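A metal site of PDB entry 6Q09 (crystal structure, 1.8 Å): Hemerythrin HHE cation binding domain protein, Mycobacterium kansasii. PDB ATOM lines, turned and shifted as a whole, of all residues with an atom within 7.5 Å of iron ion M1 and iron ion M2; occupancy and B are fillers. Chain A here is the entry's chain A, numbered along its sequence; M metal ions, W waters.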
ATOM      1  N   LEU A  16      26.983  23.265 -13.450  1.00  0.00           N
ATOM      2  CA  LEU A  16      25.534  23.095 -13.320  1.00  0.00           C
ATOM      3  C   LEU A  16      24.805  24.374 -13.703  1.00  0.00           C
ATOM      4  O   LEU A  16      23.756  24.326 -14.361  1.00  0.00           O
ATOM      5  CB  LEU A  16      25.155  22.709 -11.896  1.00  0.00           C
ATOM      6  CG  LEU A  16      25.583  21.296 -11.550  1.00  0.00           C
ATOM      7  CD1 LEU A  16      25.374  21.060 -10.077  1.00  0.00           C
ATOM      8  CD2 LEU A  16      24.798  20.286 -12.374  1.00  0.00           C
ATOM      9  N   LYS A  17      25.333  25.529 -13.301  1.00  0.00           N
ATOM     10  CA  LYS A  17      24.639  26.768 -13.642  1.00  0.00           C
ATOM     11  C   LYS A  17      24.629  27.001 -15.150  1.00  0.00           C
ATOM     12  O   LYS A  17      23.600  27.387 -15.722  1.00  0.00           O
ATOM     13  CB  LYS A  17      25.269  27.940 -12.918  1.00  0.00           C
ATOM     14  CG  LYS A  17      25.021  27.950 -11.426  1.00  0.00           C
ATOM     15  CD  LYS A  17      25.856  29.051 -10.807  1.00  0.00           C
ATOM     16  CE  LYS A  17      25.014  30.008 -10.022  1.00  0.00           C
ATOM     17  NZ  LYS A  17      25.847  31.188  -9.654  1.00  0.00           N
ATOM     18  N   HIS A  19      24.836  24.695 -17.433  1.00  0.00           N
ATOM     19  CA  HIS A  19      23.945  23.727 -18.059  1.00  0.00           C
ATOM     20  C   HIS A  19      22.490  24.089 -17.819  1.00  0.00           C
ATOM     21  O   HIS A  19      21.637  23.812 -18.678  1.00  0.00           O
ATOM     22  CB  HIS A  19      24.224  22.311 -17.559  1.00  0.00           C
ATOM     23  CG  HIS A  19      23.752  21.262 -18.509  1.00  0.00           C
ATOM     24  ND1 HIS A  19      23.041  20.157 -18.109  1.00  0.00           N
ATOM     25  CD2 HIS A  19      23.798  21.203 -19.862  1.00  0.00           C
ATOM     26  CE1 HIS A  19      22.697  19.443 -19.168  1.00  0.00           C
ATOM     27  NE2 HIS A  19      23.161  20.044 -20.244  1.00  0.00           N
ATOM     28  N   HIS A  20      22.176  24.678 -16.664  1.00  0.00           N
ATOM     29  CA  HIS A  20      20.836  25.201 -16.442  1.00  0.00           C
ATOM     30  C   HIS A  20      20.466  26.242 -17.489  1.00  0.00           C
ATOM     31  O   HIS A  20      19.328  26.257 -17.987  1.00  0.00           O
ATOM     32  CB  HIS A  20      20.716  25.816 -15.052  1.00  0.00           C
ATOM     33  CG  HIS A  20      20.557  24.818 -13.945  1.00  0.00           C
ATOM     34  ND1 HIS A  20      20.892  25.083 -12.635  1.00  0.00           N
ATOM     35  CD2 HIS A  20      20.087  23.539 -13.952  1.00  0.00           C
ATOM     36  CE1 HIS A  20      20.644  24.025 -11.889  1.00  0.00           C
ATOM     37  NE2 HIS A  20      20.159  23.077 -12.665  1.00  0.00           N
ATOM     38  N   ILE A  23      19.461  24.445 -20.566  1.00  0.00           N
ATOM     39  CA  ILE A  23      18.152  23.784 -20.484  1.00  0.00           C
ATOM     40  C   ILE A  23      17.031  24.826 -20.555  1.00  0.00           C
ATOM     41  O   ILE A  23      16.015  24.651 -21.256  1.00  0.00           O
ATOM     42  CB  ILE A  23      18.069  22.955 -19.189  1.00  0.00           C
ATOM     43  CG1 ILE A  23      18.956  21.714 -19.343  1.00  0.00           C
ATOM     44  CG2 ILE A  23      16.590  22.596 -18.857  1.00  0.00           C
ATOM     45  CD1 ILE A  23      19.247  21.022 -18.009  1.00  0.00           C
ATOM     46  N   HIS A  54      21.724  15.876 -17.412  1.00  0.00           N
ATOM     47  CA  HIS A  54      21.742  16.755 -16.253  1.00  0.00           C
ATOM     48  C   HIS A  54      21.408  16.014 -14.971  1.00  0.00           C
ATOM     49  O   HIS A  54      22.139  16.091 -13.969  1.00  0.00           O
ATOM     50  CB  HIS A  54      20.750  17.921 -16.453  1.00  0.00           C
ATOM     51  CG  HIS A  54      20.887  19.014 -15.428  1.00  0.00           C
ATOM     52  ND1 HIS A  54      21.838  20.007 -15.525  1.00  0.00           N
ATOM     53  CD2 HIS A  54      20.177  19.282 -14.306  1.00  0.00           C
ATOM     54  CE1 HIS A  54      21.708  20.834 -14.504  1.00  0.00           C
ATOM     55  NE2 HIS A  54      20.724  20.405 -13.742  1.00  0.00           N
ATOM     56  N   PHE A  55      20.308  15.275 -14.983  1.00  0.00           N
ATOM     57  CA  PHE A  55      19.935  14.582 -13.754  1.00  0.00           C
ATOM     58  C   PHE A  55      20.956  13.519 -13.420  1.00  0.00           C
ATOM     59  O   PHE A  55      21.183  13.232 -12.233  1.00  0.00           O
ATOM     60  CB  PHE A  55      18.548  13.964 -13.884  1.00  0.00           C
ATOM     61  CG  PHE A  55      17.422  14.981 -13.789  1.00  0.00           C
ATOM     62  CD1 PHE A  55      17.699  16.308 -13.464  1.00  0.00           C
ATOM     63  CD2 PHE A  55      16.112  14.598 -13.991  1.00  0.00           C
ATOM     64  CE1 PHE A  55      16.666  17.272 -13.372  1.00  0.00           C
ATOM     65  CE2 PHE A  55      15.090  15.541 -13.907  1.00  0.00           C
ATOM     66  CZ  PHE A  55      15.369  16.882 -13.592  1.00  0.00           C
ATOM     67  N   ILE A  57      24.346  13.582 -14.065  1.00  0.00           N
ATOM     68  CA  ILE A  57      25.536  14.104 -13.409  1.00  0.00           C
ATOM     69  C   ILE A  57      25.195  14.583 -12.000  1.00  0.00           C
ATOM     70  O   ILE A  57      26.040  14.450 -11.099  1.00  0.00           O
ATOM     71  CB  ILE A  57      26.246  15.186 -14.246  1.00  0.00           C
ATOM     72  CG1 ILE A  57      25.435  16.475 -14.331  1.00  0.00           C
ATOM     73  CG2 ILE A  57      26.563  14.656 -15.641  1.00  0.00           C
ATOM     74  CD1 ILE A  57      26.342  17.673 -14.338  1.00  0.00           C
ATOM     75  N   GLU A  58      23.984  15.097 -11.761  1.00  0.00           N
ATOM     76  CA  GLU A  58      23.580  15.438 -10.391  1.00  0.00           C
ATOM     77  C   GLU A  58      23.504  14.192  -9.498  1.00  0.00           C
ATOM     78  O   GLU A  58      24.097  14.152  -8.412  1.00  0.00           O
ATOM     79  CB  GLU A  58      22.252  16.240 -10.397  1.00  0.00           C
ATOM     80  CG  GLU A  58      22.506  17.635 -10.946  1.00  0.00           C
ATOM     81  CD  GLU A  58      21.266  18.477 -10.884  1.00  0.00           C
ATOM     82  OE1 GLU A  58      20.209  17.902 -10.571  1.00  0.00           O
ATOM     83  OE2 GLU A  58      21.410  19.675 -11.131  1.00  0.00           O
ATOM     84  N   ASP A  59      22.822  13.122  -9.967  1.00  0.00           N
ATOM     85  CA  ASP A  59      22.661  11.956  -9.099  1.00  0.00           C
ATOM     86  C   ASP A  59      23.976  11.250  -8.889  1.00  0.00           C
ATOM     87  O   ASP A  59      24.203  10.656  -7.825  1.00  0.00           O
ATOM     88  CB  ASP A  59      21.691  10.943  -9.697  1.00  0.00           C
ATOM     89  CG  ASP A  59      20.275  11.443  -9.759  1.00  0.00           C
ATOM     90  OD1 ASP A  59      19.954  12.406  -9.036  1.00  0.00           O
ATOM     91  OD2 ASP A  59      19.502  10.859 -10.540  1.00  0.00           O
ATOM     92  N   TYR A  62      27.272  15.041  -8.322  1.00  0.00           N
ATOM     93  CA  TYR A  62      27.114  16.266  -7.541  1.00  0.00           C
ATOM     94  C   TYR A  62      26.457  15.996  -6.192  1.00  0.00           C
ATOM     95  O   TYR A  62      26.983  16.391  -5.149  1.00  0.00           O
ATOM     96  CB  TYR A  62      26.300  17.302  -8.314  1.00  0.00           C
ATOM     97  CG  TYR A  62      26.303  18.667  -7.622  1.00  0.00           C
ATOM     98  CD1 TYR A  62      27.468  19.403  -7.508  1.00  0.00           C
ATOM     99  CD2 TYR A  62      25.107  19.215  -7.097  1.00  0.00           C
ATOM    100  CE1 TYR A  62      27.489  20.633  -6.882  1.00  0.00           C
ATOM    101  CE2 TYR A  62      25.110  20.479  -6.488  1.00  0.00           C
ATOM    102  CZ  TYR A  62      26.296  21.174  -6.387  1.00  0.00           C
ATOM    103  OH  TYR A  62      26.351  22.391  -5.773  1.00  0.00           O
ATOM    104  N   TYR A  63      25.300  15.346  -6.200  1.00  0.00           N
ATOM    105  CA  TYR A  63      24.624  15.101  -4.940  1.00  0.00           C
ATOM    106  C   TYR A  63      25.444  14.211  -4.010  1.00  0.00           C
ATOM    107  O   TYR A  63      25.469  14.489  -2.804  1.00  0.00           O
ATOM    108  CB  TYR A  63      23.234  14.495  -5.164  1.00  0.00           C
ATOM    109  CG  TYR A  63      22.236  15.419  -5.824  1.00  0.00           C
ATOM    110  CD1 TYR A  63      22.411  16.785  -5.833  1.00  0.00           C
ATOM    111  CD2 TYR A  63      21.094  14.900  -6.445  1.00  0.00           C
ATOM    112  CE1 TYR A  63      21.478  17.641  -6.452  1.00  0.00           C
ATOM    113  CE2 TYR A  63      20.170  15.715  -7.040  1.00  0.00           C
ATOM    114  CZ  TYR A  63      20.373  17.082  -7.041  1.00  0.00           C
ATOM    115  OH  TYR A  63      19.437  17.868  -7.639  1.00  0.00           O
ATOM    116  N   ALA A  76      15.880  17.091  -3.115  1.00  0.00           N
ATOM    117  CA  ALA A  76      16.315  17.189  -4.509  1.00  0.00           C
ATOM    118  C   ALA A  76      15.996  15.923  -5.296  1.00  0.00           C
ATOM    119  O   ALA A  76      15.546  15.989  -6.444  1.00  0.00           O
ATOM    120  CB  ALA A  76      17.809  17.504  -4.565  1.00  0.00           C
ATOM    121  N   HIS A  77      16.227  14.740  -4.698  1.00  0.00           N
ATOM    122  CA  HIS A  77      15.803  13.507  -5.360  1.00  0.00           C
ATOM    123  C   HIS A  77      14.291  13.476  -5.562  1.00  0.00           C
ATOM    124  O   HIS A  77      13.807  12.970  -6.581  1.00  0.00           O
ATOM    125  CB  HIS A  77      16.266  12.295  -4.546  1.00  0.00           C
ATOM    126  CG  HIS A  77      17.711  11.997  -4.737  1.00  0.00           C
ATOM    127  ND1 HIS A  77      18.558  11.719  -3.698  1.00  0.00           N
ATOM    128  CD2 HIS A  77      18.460  11.915  -5.869  1.00  0.00           C
ATOM    129  CE1 HIS A  77      19.773  11.505  -4.168  1.00  0.00           C
ATOM    130  NE2 HIS A  77      19.747  11.607  -5.481  1.00  0.00           N
ATOM    131  N   GLU A  79      12.365  16.101  -5.979  1.00  0.00           N
ATOM    132  CA  GLU A  79      12.051  17.009  -7.070  1.00  0.00           C
ATOM    133  C   GLU A  79      12.412  16.418  -8.430  1.00  0.00           C
ATOM    134  O   GLU A  79      11.712  16.675  -9.414  1.00  0.00           O
ATOM    135  CB  GLU A  79      12.762  18.337  -6.865  1.00  0.00           C
ATOM    136  CG  GLU A  79      12.430  18.936  -5.528  1.00  0.00           C
ATOM    137  CD  GLU A  79      12.355  20.433  -5.560  1.00  0.00           C
ATOM    138  OE1 GLU A  79      13.103  21.050  -6.352  1.00  0.00           O
ATOM    139  OE2 GLU A  79      11.511  20.971  -4.824  1.00  0.00           O
ATOM    140  N   HIS A  80      13.486  15.604  -8.510  1.00  0.00           N
ATOM    141  CA  HIS A  80      13.755  14.933  -9.772  1.00  0.00           C
ATOM    142  C   HIS A  80      12.591  14.015 -10.136  1.00  0.00           C
ATOM    143  O   HIS A  80      12.192  13.935 -11.309  1.00  0.00           O
ATOM    144  CB  HIS A  80      15.077  14.153  -9.726  1.00  0.00           C
ATOM    145  CG  HIS A  80      16.282  15.036  -9.840  1.00  0.00           C
ATOM    146  ND1 HIS A  80      17.555  14.539 -10.040  1.00  0.00           N
ATOM    147  CD2 HIS A  80      16.399  16.380  -9.772  1.00  0.00           C
ATOM    148  CE1 HIS A  80      18.403  15.557 -10.095  1.00  0.00           C
ATOM    149  NE2 HIS A  80      17.725  16.679  -9.930  1.00  0.00           N
ATOM    150  N   VAL A  83       9.742  16.078 -11.702  1.00  0.00           N
ATOM    151  CA  VAL A  83       9.995  16.366 -13.111  1.00  0.00           C
ATOM    152  C   VAL A  83       9.756  15.130 -13.968  1.00  0.00           C
ATOM    153  O   VAL A  83       9.113  15.204 -15.017  1.00  0.00           O
ATOM    154  CB  VAL A  83      11.418  16.910 -13.283  1.00  0.00           C
ATOM    155  CG1 VAL A  83      11.729  17.108 -14.746  1.00  0.00           C
ATOM    156  CG2 VAL A  83      11.589  18.198 -12.499  1.00  0.00           C
ATOM    157  N   LEU A 111       9.744  21.860 -14.014  1.00  0.00           N
ATOM    158  CA  LEU A 111      11.178  21.766 -14.273  1.00  0.00           C
ATOM    159  C   LEU A 111      11.900  23.035 -13.824  1.00  0.00           C
ATOM    160  O   LEU A 111      12.919  22.977 -13.122  1.00  0.00           O
ATOM    161  CB  LEU A 111      11.416  21.493 -15.766  1.00  0.00           C
ATOM    162  CG  LEU A 111      12.866  21.515 -16.271  1.00  0.00           C
ATOM    163  CD1 LEU A 111      13.705  20.437 -15.574  1.00  0.00           C
ATOM    164  CD2 LEU A 111      12.903  21.339 -17.772  1.00  0.00           C
ATOM    165  N   HIS A 114      12.126  23.365  -9.917  1.00  0.00           N
ATOM    166  CA  HIS A 114      13.223  22.542  -9.405  1.00  0.00           C
ATOM    167  C   HIS A 114      14.569  23.238  -9.591  1.00  0.00           C
ATOM    168  O   HIS A 114      15.334  23.393  -8.642  1.00  0.00           O
ATOM    169  CB  HIS A 114      13.231  21.177 -10.083  1.00  0.00           C
ATOM    170  CG  HIS A 114      14.568  20.512 -10.002  1.00  0.00           C
ATOM    171  ND1 HIS A 114      15.131  20.104  -8.808  1.00  0.00           N
ATOM    172  CD2 HIS A 114      15.480  20.241 -10.959  1.00  0.00           C
ATOM    173  CE1 HIS A 114      16.313  19.575  -9.045  1.00  0.00           C
ATOM    174  NE2 HIS A 114      16.550  19.645 -10.342  1.00  0.00           N
ATOM    175  N   ALA A 115      14.859  23.665 -10.822  1.00  0.00           N
ATOM    176  CA  ALA A 115      16.171  24.274 -11.080  1.00  0.00           C
ATOM    177  C   ALA A 115      16.380  25.536 -10.274  1.00  0.00           C
ATOM    178  O   ALA A 115      17.512  25.866  -9.884  1.00  0.00           O
ATOM    179  CB  ALA A 115      16.346  24.557 -12.574  1.00  0.00           C
ATOM    180  N   ASP A 116      15.309  26.269  -9.994  1.00  0.00           N
ATOM    181  CA  ASP A 116      15.447  27.451  -9.156  1.00  0.00           C
ATOM    182  C   ASP A 116      15.625  27.068  -7.691  1.00  0.00           C
ATOM    183  O   ASP A 116      16.430  27.680  -6.973  1.00  0.00           O
ATOM    184  CB  ASP A 116      14.255  28.382  -9.342  1.00  0.00           C
ATOM    185  CG  ASP A 116      14.233  29.064 -10.710  1.00  0.00           C
ATOM    186  OD1 ASP A 116      15.300  29.159 -11.351  1.00  0.00           O
ATOM    187  OD2 ASP A 116      13.152  29.514 -11.141  1.00  0.00           O
ATOM    188  N   GLU A 118      16.979  24.395  -6.715  1.00  0.00           N
ATOM    189  CA  GLU A 118      18.357  23.907  -6.675  1.00  0.00           C
ATOM    190  C   GLU A 118      19.342  25.055  -6.491  1.00  0.00           C
ATOM    191  O   GLU A 118      20.211  25.015  -5.615  1.00  0.00           O
ATOM    192  CB  GLU A 118      18.643  23.173  -7.963  1.00  0.00           C
ATOM    193  CG  GLU A 118      19.813  22.266  -7.951  1.00  0.00           C
ATOM    194  CD  GLU A 118      19.722  21.320  -9.131  1.00  0.00           C
ATOM    195  OE1 GLU A 118      20.050  21.780 -10.247  1.00  0.00           O
ATOM    196  OE2 GLU A 118      19.260  20.172  -8.938  1.00  0.00           O
ATOM    197  N   GLU A 119      19.216  26.118  -7.298  1.00  0.00           N
ATOM    198  CA  GLU A 119      20.100  27.262  -7.124  1.00  0.00           C
ATOM    199  C   GLU A 119      19.814  28.053  -5.847  1.00  0.00           C
ATOM    200  O   GLU A 119      20.591  28.947  -5.494  1.00  0.00           O
ATOM    201  CB  GLU A 119      20.040  28.171  -8.348  1.00  0.00           C
ATOM    202  CG  GLU A 119      20.997  27.709  -9.447  1.00  0.00           C
ATOM    203  CD  GLU A 119      20.681  28.265 -10.798  1.00  0.00           C
ATOM    204  OE1 GLU A 119      19.968  29.289 -10.872  1.00  0.00           O
ATOM    205  OE2 GLU A 119      21.162  27.693 -11.798  1.00  0.00           O
ATOM    206  N   ILE A 123      23.244  25.159  -4.613  1.00  0.00           N
ATOM    207  CA  ILE A 123      24.381  25.809  -5.278  1.00  0.00           C
ATOM    208  C   ILE A 123      24.574  27.187  -4.655  1.00  0.00           C
ATOM    209  O   ILE A 123      23.717  28.069  -4.844  1.00  0.00           O
ATOM    210  CB  ILE A 123      24.182  25.900  -6.800  1.00  0.00           C
ATOM    211  CG1 ILE A 123      23.965  24.499  -7.410  1.00  0.00           C
ATOM    212  CG2 ILE A 123      25.362  26.601  -7.443  1.00  0.00           C
ATOM    213  CD1 ILE A 123      23.574  24.505  -8.894  1.00  0.00           C
HETATM  214 FE    FE M   1      20.049  21.010 -12.048  1.00  0.00          FE
HETATM  215 FE    FE M   2      18.458  18.919 -10.236  1.00  0.00          FE
HETATM  216  O   HOH W   1      18.437  20.467 -12.183  1.00  0.00           O
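OE2 of Glu 119 sits at hydrogen-bond distance from ND1 of His 20. A ring nitrogen (ND1) of His 20 lies close to the backbone carbonyl oxygen (O) of Leu 16 (3.4 Å). The side-chain hydroxyl (OH) of Tyr 63 sits close to a ring nitrogen (NE2) of His 80. OE2 of Glu 118 sits close to OH of Tyr 63 (2.7 Å). ND1 of His 54 sits at hydrogen-bond distance from ND1 of His 19, at 2.9 Å. The backbone carbonyl oxygen (O) of Glu 118 is in hydrogen-bond range of the backbone NH (N) of Ile 123 (3.2 Å). A ring nitrogen (ND1) of His 114 is in hydrogen-bond range of the side-chain carboxylate of Glu 79, at 3.3 Å. N of Tyr 63 is in hydrogen-bond range of O of Glu 58 (2.8 Å).
Within 4 Å of iron ion M1: His 20, His 54, Glu 58 and Glu 118. The nearest printed residue that does not touch iron ion M1 is His 114 (4.1 Å).
Residues that only touch iron ion M2: Phe 55 and Tyr 63. Six residues have an atom within 4 Å of iron ion M2: Phe 55, Glu 58, Tyr 63, His 80, His 114 and Glu 118.
Iron ion M1 is bound by water W1 (1.7 Å). Iron ion M1 is bound by NE2 of His 54 (1.9 Å). OE1 of Glu 118 binds iron ion M1, at 2.0 Å. OE2 of Glu 58 binds iron ion M1 (2.1 Å). NE2 of His 20 is bound to iron ion M1, 2.2 Å away.
Iron ion M2 is bound by the side-chain carboxylate (OE2) of Glu 118 (2.0 Å), a ring nitrogen (NE2) of His 114 (2.0 Å), the side-chain carboxylate (OE1) of Glu 58 (2.1 Å), a ring nitrogen (NE2) of His 80 (2.4 Å) and water W1 (2.5 Å).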
